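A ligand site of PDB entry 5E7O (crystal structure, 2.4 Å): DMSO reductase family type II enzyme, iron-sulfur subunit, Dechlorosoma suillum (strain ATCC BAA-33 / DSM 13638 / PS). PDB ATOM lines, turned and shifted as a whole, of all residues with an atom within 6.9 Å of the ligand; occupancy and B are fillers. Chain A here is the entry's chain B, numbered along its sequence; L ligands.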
ATOM      1  N   GLY A  67      17.274  21.229 -34.044  1.00  0.00           N
ATOM      2  CA  GLY A  67      16.390  21.378 -32.895  1.00  0.00           C
ATOM      3  C   GLY A  67      15.816  20.042 -32.478  1.00  0.00           C
ATOM      4  O   GLY A  67      16.557  19.068 -32.294  1.00  0.00           O
ATOM      5  N   MET A 136      21.594  35.560 -31.639  1.00  0.00           N
ATOM      6  CA  MET A 136      22.808  35.131 -30.951  1.00  0.00           C
ATOM      7  C   MET A 136      22.609  33.669 -30.575  1.00  0.00           C
ATOM      8  O   MET A 136      21.586  33.057 -30.899  1.00  0.00           O
ATOM      9  CB  MET A 136      23.080  35.986 -29.715  1.00  0.00           C
ATOM     10  CG  MET A 136      21.891  36.071 -28.778  1.00  0.00           C
ATOM     11  SD  MET A 136      22.160  37.146 -27.347  1.00  0.00           S
ATOM     12  CE  MET A 136      23.568  36.336 -26.588  1.00  0.00           C
ATOM     13  N   CYS A 137      23.598  33.116 -29.904  1.00  0.00           N
ATOM     14  CA  CYS A 137      23.436  31.798 -29.318  1.00  0.00           C
ATOM     15  C   CYS A 137      22.424  31.840 -28.179  1.00  0.00           C
ATOM     16  O   CYS A 137      22.533  32.664 -27.268  1.00  0.00           O
ATOM     17  CB  CYS A 137      24.769  31.284 -28.805  1.00  0.00           C
ATOM     18  SG  CYS A 137      24.567  30.053 -27.509  1.00  0.00           S
ATOM     19  N   ASN A 138      21.436  30.942 -28.233  1.00  0.00           N
ATOM     20  CA  ASN A 138      20.350  30.972 -27.273  1.00  0.00           C
ATOM     21  C   ASN A 138      20.713  30.345 -25.930  1.00  0.00           C
ATOM     22  O   ASN A 138      19.953  30.495 -24.969  1.00  0.00           O
ATOM     23  CB  ASN A 138      19.118  30.259 -27.849  1.00  0.00           C
ATOM     24  CG  ASN A 138      18.692  30.836 -29.185  1.00  0.00           C
ATOM     25  OD1 ASN A 138      17.831  31.712 -29.256  1.00  0.00           O
ATOM     26  ND2 ASN A 138      19.302  30.351 -30.264  1.00  0.00           N
ATOM     27  N   HIS A 139      21.861  29.664 -25.842  1.00  0.00           N
ATOM     28  CA  HIS A 139      22.285  28.965 -24.627  1.00  0.00           C
ATOM     29  C   HIS A 139      21.149  28.121 -24.065  1.00  0.00           C
ATOM     30  O   HIS A 139      20.779  28.218 -22.897  1.00  0.00           O
ATOM     31  CB  HIS A 139      22.808  29.958 -23.584  1.00  0.00           C
ATOM     32  CG  HIS A 139      23.939  30.814 -24.073  1.00  0.00           C
ATOM     33  ND1 HIS A 139      25.236  30.357 -24.132  1.00  0.00           N
ATOM     34  CD2 HIS A 139      23.969  32.090 -24.520  1.00  0.00           C
ATOM     35  CE1 HIS A 139      26.019  31.323 -24.600  1.00  0.00           C
ATOM     36  NE2 HIS A 139      25.267  32.379 -24.842  1.00  0.00           N
ATOM     37  N   CYS A 140      20.594  27.281 -24.939  1.00  0.00           N
ATOM     38  CA  CYS A 140      19.345  26.597 -24.653  1.00  0.00           C
ATOM     39  C   CYS A 140      19.475  25.647 -23.458  1.00  0.00           C
ATOM     40  O   CYS A 140      20.553  25.101 -23.192  1.00  0.00           O
ATOM     41  CB  CYS A 140      18.864  25.821 -25.876  1.00  0.00           C
ATOM     42  SG  CYS A 140      18.280  26.844 -27.240  1.00  0.00           S
ATOM     43  N   THR A 141      18.361  25.456 -22.758  1.00  0.00           N
ATOM     44  CA  THR A 141      18.289  24.442 -21.707  1.00  0.00           C
ATOM     45  C   THR A 141      18.389  23.039 -22.284  1.00  0.00           C
ATOM     46  O   THR A 141      18.802  22.114 -21.580  1.00  0.00           O
ATOM     47  CB  THR A 141      17.007  24.614 -20.895  1.00  0.00           C
ATOM     48  OG1 THR A 141      16.892  25.983 -20.460  1.00  0.00           O
ATOM     49  CG2 THR A 141      16.987  23.702 -19.689  1.00  0.00           C
ATOM     50  N   LYS A 142      18.025  22.858 -23.560  1.00  0.00           N
ATOM     51  CA  LYS A 142      18.199  21.602 -24.283  1.00  0.00           C
ATOM     52  C   LYS A 142      19.043  21.890 -25.522  1.00  0.00           C
ATOM     53  O   LYS A 142      18.512  21.941 -26.642  1.00  0.00           O
ATOM     54  CB  LYS A 142      16.862  20.971 -24.663  1.00  0.00           C
ATOM     55  CG  LYS A 142      16.896  19.458 -24.842  1.00  0.00           C
ATOM     56  CD  LYS A 142      15.512  18.907 -25.127  1.00  0.00           C
ATOM     57  CE  LYS A 142      15.498  17.387 -25.037  1.00  0.00           C
ATOM     58  NZ  LYS A 142      15.850  16.917 -23.668  1.00  0.00           N
ATOM     59  N   PRO A 143      20.352  22.099 -25.356  1.00  0.00           N
ATOM     60  CA  PRO A 143      21.195  22.468 -26.505  1.00  0.00           C
ATOM     61  C   PRO A 143      21.284  21.327 -27.508  1.00  0.00           C
ATOM     62  O   PRO A 143      21.789  20.238 -27.192  1.00  0.00           O
ATOM     63  CB  PRO A 143      22.558  22.763 -25.851  1.00  0.00           C
ATOM     64  CG  PRO A 143      22.531  22.005 -24.571  1.00  0.00           C
ATOM     65  CD  PRO A 143      21.109  22.023 -24.099  1.00  0.00           C
ATOM     66  N   ALA A 144      20.799  21.576 -28.715  1.00  0.00           N
ATOM     67  CA  ALA A 144      20.833  20.550 -29.762  1.00  0.00           C
ATOM     68  C   ALA A 144      22.240  20.330 -30.293  1.00  0.00           C
ATOM     69  O   ALA A 144      22.559  19.240 -30.772  1.00  0.00           O
ATOM     70  CB  ALA A 144      19.888  20.934 -30.900  1.00  0.00           C
ATOM     71  N   CYS A 145      23.090  21.357 -30.229  1.00  0.00           N
ATOM     72  CA  CYS A 145      24.479  21.205 -30.631  1.00  0.00           C
ATOM     73  C   CYS A 145      25.205  20.222 -29.719  1.00  0.00           C
ATOM     74  O   CYS A 145      25.849  19.279 -30.182  1.00  0.00           O
ATOM     75  CB  CYS A 145      25.193  22.555 -30.610  1.00  0.00           C
ATOM     76  SG  CYS A 145      25.616  23.111 -28.933  1.00  0.00           S
ATOM     77  N   LEU A 146      25.112  20.459 -28.410  1.00  0.00           N
ATOM     78  CA  LEU A 146      25.712  19.565 -27.417  1.00  0.00           C
ATOM     79  C   LEU A 146      25.214  18.140 -27.583  1.00  0.00           C
ATOM     80  O   LEU A 146      25.984  17.185 -27.440  1.00  0.00           O
ATOM     81  CB  LEU A 146      25.392  20.081 -26.011  1.00  0.00           C
ATOM     82  CG  LEU A 146      25.734  19.227 -24.804  1.00  0.00           C
ATOM     83  CD1 LEU A 146      27.204  18.932 -24.753  1.00  0.00           C
ATOM     84  CD2 LEU A 146      25.276  19.921 -23.540  1.00  0.00           C
ATOM     85  N   ILE A 154      31.358  19.967 -27.138  1.00  0.00           N
ATOM     86  CA  ILE A 154      30.568  21.019 -26.533  1.00  0.00           C
ATOM     87  C   ILE A 154      30.190  20.621 -25.112  1.00  0.00           C
ATOM     88  O   ILE A 154      30.201  19.443 -24.741  1.00  0.00           O
ATOM     89  CB  ILE A 154      29.337  21.295 -27.401  1.00  0.00           C
ATOM     90  CG1 ILE A 154      29.790  21.535 -28.847  1.00  0.00           C
ATOM     91  CG2 ILE A 154      28.542  22.494 -26.904  1.00  0.00           C
ATOM     92  CD1 ILE A 154      28.687  21.886 -29.802  1.00  0.00           C
ATOM     93  N   LYS A 156      27.838  22.341 -21.452  1.00  0.00           N
ATOM     94  CA  LYS A 156      27.060  23.376 -20.798  1.00  0.00           C
ATOM     95  C   LYS A 156      27.573  23.562 -19.374  1.00  0.00           C
ATOM     96  O   LYS A 156      27.646  22.595 -18.609  1.00  0.00           O
ATOM     97  CB  LYS A 156      25.568  23.030 -20.782  1.00  0.00           C
ATOM     98  CG  LYS A 156      24.667  24.149 -20.287  1.00  0.00           C
ATOM     99  CD  LYS A 156      23.208  23.701 -20.306  1.00  0.00           C
ATOM    100  CE  LYS A 156      22.279  24.868 -20.009  1.00  0.00           C
ATOM    101  NZ  LYS A 156      21.758  25.507 -21.245  1.00  0.00           N
ATOM    102  N   VAL A 163      26.645  27.838 -22.900  1.00  0.00           N
ATOM    103  CA  VAL A 163      27.118  26.739 -23.737  1.00  0.00           C
ATOM    104  C   VAL A 163      28.375  27.207 -24.466  1.00  0.00           C
ATOM    105  O   VAL A 163      28.375  28.267 -25.106  1.00  0.00           O
ATOM    106  CB  VAL A 163      26.031  26.284 -24.725  1.00  0.00           C
ATOM    107  CG1 VAL A 163      26.579  25.239 -25.685  1.00  0.00           C
ATOM    108  CG2 VAL A 163      24.822  25.739 -23.979  1.00  0.00           C
ATOM    109  N   ILE A 165      31.812  25.671 -26.822  1.00  0.00           N
ATOM    110  CA  ILE A 165      32.454  24.576 -27.535  1.00  0.00           C
ATOM    111  C   ILE A 165      33.926  24.542 -27.112  1.00  0.00           C
ATOM    112  O   ILE A 165      34.650  25.529 -27.270  1.00  0.00           O
ATOM    113  CB  ILE A 165      32.325  24.750 -29.055  1.00  0.00           C
ATOM    114  CG1 ILE A 165      30.863  24.966 -29.443  1.00  0.00           C
ATOM    115  CG2 ILE A 165      32.888  23.529 -29.775  1.00  0.00           C
ATOM    116  CD1 ILE A 165      30.639  25.085 -30.931  1.00  0.00           C
ATOM    117  N   CYS A 176      27.058  19.707 -34.735  1.00  0.00           N
ATOM    118  CA  CYS A 176      26.407  20.825 -34.048  1.00  0.00           C
ATOM    119  C   CYS A 176      25.812  21.805 -35.054  1.00  0.00           C
ATOM    120  O   CYS A 176      24.731  22.364 -34.816  1.00  0.00           O
ATOM    121  CB  CYS A 176      27.410  21.535 -33.150  1.00  0.00           C
ATOM    122  SG  CYS A 176      28.692  22.428 -34.058  1.00  0.00           S
ATOM    123  N   SER A 179      22.548  20.244 -36.437  1.00  0.00           N
ATOM    124  CA  SER A 179      21.428  20.052 -35.520  1.00  0.00           C
ATOM    125  C   SER A 179      21.013  21.320 -34.782  1.00  0.00           C
ATOM    126  O   SER A 179      19.967  21.308 -34.116  1.00  0.00           O
ATOM    127  CB  SER A 179      21.767  18.958 -34.504  1.00  0.00           C
ATOM    128  OG  SER A 179      21.864  17.686 -35.142  1.00  0.00           O
ATOM    129  N   CYS A 180      21.792  22.382 -34.858  1.00  0.00           N
ATOM    130  CA  CYS A 180      21.346  23.655 -34.321  1.00  0.00           C
ATOM    131  C   CYS A 180      20.348  24.287 -35.289  1.00  0.00           C
ATOM    132  O   CYS A 180      20.706  24.546 -36.446  1.00  0.00           O
ATOM    133  CB  CYS A 180      22.505  24.605 -34.104  1.00  0.00           C
ATOM    134  SG  CYS A 180      21.941  26.273 -33.663  1.00  0.00           S
ATOM    135  N   PRO A 181      19.117  24.556 -34.866  1.00  0.00           N
ATOM    136  CA  PRO A 181      18.133  25.154 -35.769  1.00  0.00           C
ATOM    137  C   PRO A 181      18.261  26.663 -35.907  1.00  0.00           C
ATOM    138  O   PRO A 181      17.493  27.260 -36.669  1.00  0.00           O
ATOM    139  CB  PRO A 181      16.806  24.769 -35.112  1.00  0.00           C
ATOM    140  CG  PRO A 181      17.129  24.768 -33.647  1.00  0.00           C
ATOM    141  CD  PRO A 181      18.550  24.283 -33.531  1.00  0.00           C
ATOM    142  N   TYR A 182      19.182  27.291 -35.192  1.00  0.00           N
ATOM    143  CA  TYR A 182      19.395  28.730 -35.268  1.00  0.00           C
ATOM    144  C   TYR A 182      20.643  29.102 -36.061  1.00  0.00           C
ATOM    145  O   TYR A 182      20.890  30.295 -36.283  1.00  0.00           O
ATOM    146  CB  TYR A 182      19.474  29.329 -33.863  1.00  0.00           C
ATOM    147  CG  TYR A 182      18.240  29.061 -33.042  1.00  0.00           C
ATOM    148  CD1 TYR A 182      17.108  29.863 -33.162  1.00  0.00           C
ATOM    149  CD2 TYR A 182      18.196  28.001 -32.139  1.00  0.00           C
ATOM    150  CE1 TYR A 182      15.980  29.622 -32.414  1.00  0.00           C
ATOM    151  CE2 TYR A 182      17.065  27.753 -31.385  1.00  0.00           C
ATOM    152  CZ  TYR A 182      15.963  28.566 -31.524  1.00  0.00           C
ATOM    153  OH  TYR A 182      14.837  28.318 -30.783  1.00  0.00           O
ATOM    154  N   ALA A 183      21.429  28.107 -36.493  1.00  0.00           N
ATOM    155  CA  ALA A 183      22.618  28.330 -37.324  1.00  0.00           C
ATOM    156  C   ALA A 183      23.604  29.280 -36.644  1.00  0.00           C
ATOM    157  O   ALA A 183      24.168  30.177 -37.269  1.00  0.00           O
ATOM    158  CB  ALA A 183      22.237  28.854 -38.711  1.00  0.00           C
ATOM    159  N   LYS A 184      23.823  29.063 -35.347  1.00  0.00           N
ATOM    160  CA  LYS A 184      24.714  29.905 -34.566  1.00  0.00           C
ATOM    161  C   LYS A 184      26.094  29.277 -34.330  1.00  0.00           C
ATOM    162  O   LYS A 184      27.044  30.010 -34.003  1.00  0.00           O
ATOM    163  CB  LYS A 184      24.067  30.267 -33.230  1.00  0.00           C
ATOM    164  CG  LYS A 184      23.200  31.523 -33.325  1.00  0.00           C
ATOM    165  CD  LYS A 184      24.035  32.696 -33.803  1.00  0.00           C
ATOM    166  CE  LYS A 184      23.199  33.740 -34.515  1.00  0.00           C
ATOM    167  NZ  LYS A 184      24.034  34.872 -35.008  1.00  0.00           N
ATOM    168  N   PRO A 185      26.262  27.959 -34.428  1.00  0.00           N
ATOM    169  CA  PRO A 185      27.621  27.413 -34.570  1.00  0.00           C
ATOM    170  C   PRO A 185      28.121  27.563 -35.998  1.00  0.00           C
ATOM    171  O   PRO A 185      27.384  27.374 -36.969  1.00  0.00           O
ATOM    172  CB  PRO A 185      27.463  25.933 -34.194  1.00  0.00           C
ATOM    173  CG  PRO A 185      26.220  25.881 -33.391  1.00  0.00           C
ATOM    174  CD  PRO A 185      25.320  26.906 -33.997  1.00  0.00           C
ATOM    175  N   LYS A 196      31.584  29.379 -31.868  1.00  0.00           N
ATOM    176  CA  LYS A 196      30.242  29.791 -31.501  1.00  0.00           C
ATOM    177  C   LYS A 196      30.341  30.880 -30.443  1.00  0.00           C
ATOM    178  O   LYS A 196      31.393  31.077 -29.822  1.00  0.00           O
ATOM    179  CB  LYS A 196      29.424  28.580 -31.024  1.00  0.00           C
ATOM    180  CG  LYS A 196      28.436  28.834 -29.906  1.00  0.00           C
ATOM    181  CD  LYS A 196      28.003  27.538 -29.278  1.00  0.00           C
ATOM    182  CE  LYS A 196      27.374  27.792 -27.942  1.00  0.00           C
ATOM    183  NZ  LYS A 196      25.902  27.912 -28.047  1.00  0.00           N
ATOM    184  N   CYS A 197      29.254  31.630 -30.297  1.00  0.00           N
ATOM    185  CA  CYS A 197      29.119  32.565 -29.183  1.00  0.00           C
ATOM    186  C   CYS A 197      29.401  31.890 -27.841  1.00  0.00           C
ATOM    187  O   CYS A 197      28.895  30.809 -27.549  1.00  0.00           O
ATOM    188  CB  CYS A 197      27.711  33.143 -29.188  1.00  0.00           C
ATOM    189  SG  CYS A 197      27.205  33.726 -27.549  1.00  0.00           S
ATOM    190  N   THR A 252      14.214  23.108 -28.293  1.00  0.00           N
ATOM    191  CA  THR A 252      15.455  23.300 -27.549  1.00  0.00           C
ATOM    192  C   THR A 252      15.279  24.177 -26.315  1.00  0.00           C
ATOM    193  O   THR A 252      16.154  24.155 -25.443  1.00  0.00           O
ATOM    194  CB  THR A 252      16.521  23.939 -28.455  1.00  0.00           C
ATOM    195  OG1 THR A 252      16.196  25.311 -28.695  1.00  0.00           O
ATOM    196  CG2 THR A 252      16.599  23.198 -29.779  1.00  0.00           C
ATOM    197  N   GLU A 253      14.180  24.923 -26.226  1.00  0.00           N
ATOM    198  CA  GLU A 253      13.895  25.833 -25.123  1.00  0.00           C
ATOM    199  C   GLU A 253      15.019  26.854 -24.987  1.00  0.00           C
ATOM    200  O   GLU A 253      15.978  26.628 -24.236  1.00  0.00           O
ATOM    201  CB  GLU A 253      13.705  25.063 -23.814  1.00  0.00           C
ATOM    202  CG  GLU A 253      12.603  24.014 -23.874  1.00  0.00           C
ATOM    203  CD  GLU A 253      12.528  23.177 -22.612  1.00  0.00           C
ATOM    204  OE1 GLU A 253      13.259  23.479 -21.643  1.00  0.00           O
ATOM    205  OE2 GLU A 253      11.748  22.195 -22.588  1.00  0.00           O
ATOM    206  N   PRO A 254      14.959  27.968 -25.710  1.00  0.00           N
ATOM    207  CA  PRO A 254      16.023  28.977 -25.620  1.00  0.00           C
ATOM    208  C   PRO A 254      15.991  29.721 -24.301  1.00  0.00           C
ATOM    209  O   PRO A 254      14.970  29.805 -23.611  1.00  0.00           O
ATOM    210  CB  PRO A 254      15.730  29.916 -26.784  1.00  0.00           C
ATOM    211  CG  PRO A 254      14.808  29.147 -27.690  1.00  0.00           C
ATOM    212  CD  PRO A 254      14.005  28.279 -26.791  1.00  0.00           C
HETATM  213 FE1  LIG L   1      22.020  26.619 -31.367  1.00  0.00          FE
HETATM  214 FE2  LIG L   1      23.355  24.761 -29.278  1.00  0.00          FE
HETATM  215 FE3  LIG L   1      20.803  26.339 -28.524  1.00  0.00          FE
HETATM  216 FE4  LIG L   1      23.470  27.819 -28.965  1.00  0.00          FE
HETATM  217  S1  LIG L   1      22.813  26.170 -27.689  1.00  0.00           S
HETATM  218  S2  LIG L   1      21.445  28.010 -29.783  1.00  0.00           S
HETATM  219  S3  LIG L   1      24.029  26.415 -30.541  1.00  0.00           S
HETATM  220  S4  LIG L   1      21.351  24.945 -30.126  1.00  0.00           S
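Cys 137 touches the ligand (SG to FE4, 2.9 Å).
N of His 139 touches FE4 of the ligand, 3.97 Å away.
Pro 143 touches the ligand (CB to S1, 3.9 Å).
SG of Cys 145 touches FE2 of the ligand, 2.8 Å away.
Pro 185 touches the ligand.
The nearest printed residue that does not touch the ligand is Tyr 182 (4.01 Å).
N of Asn 138 sits close to S2 of the ligand (3.3 Å).
The side-chain amide nitrogen (ND2) of Asn 138 lies close to a sulfur (S2) of the ligand, 3.2 Å away.
A sulfur (S4) of the ligand lies close to the backbone NH of Ala 144 (3.7 Å).
SG of Cys 180 binds FE1 of the ligand (2.3 Å).
The side-chain amino group (NZ) of Lys 196 sits close to a sulfur (S3) of the ligand.
A sulfur (S1) of the ligand lies close to the backbone NH of Cys 140 (3.7 Å).
The side-chain sulfur (SG) of Cys 140 is in hydrogen-bond range of the side-chain hydroxyl (OG1) of Thr 252 (3.0 Å).
SG of Cys 197 lies close to NE2 of His 139, 3.6 Å away.
SG of Cys 180 sits close to N of Tyr 182 (3.3 Å).
NZ of Lys 196 sits at hydrogen-bond distance from SG of Cys 137, 2.6 Å away.
The side-chain sulfur of Cys 180 sits close to the backbone NH of Lys 184 (3.8 Å).
N of Ala 183 sits close to SG of Cys 180, at 3.4 Å.
The backbone NH of Val 163 is in hydrogen-bond range of a ring nitrogen (ND1) of His 139, at 3.1 Å.
The backbone NH of His 139 is in hydrogen-bond range of the side-chain sulfur of Cys 137, at 3.2 Å.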
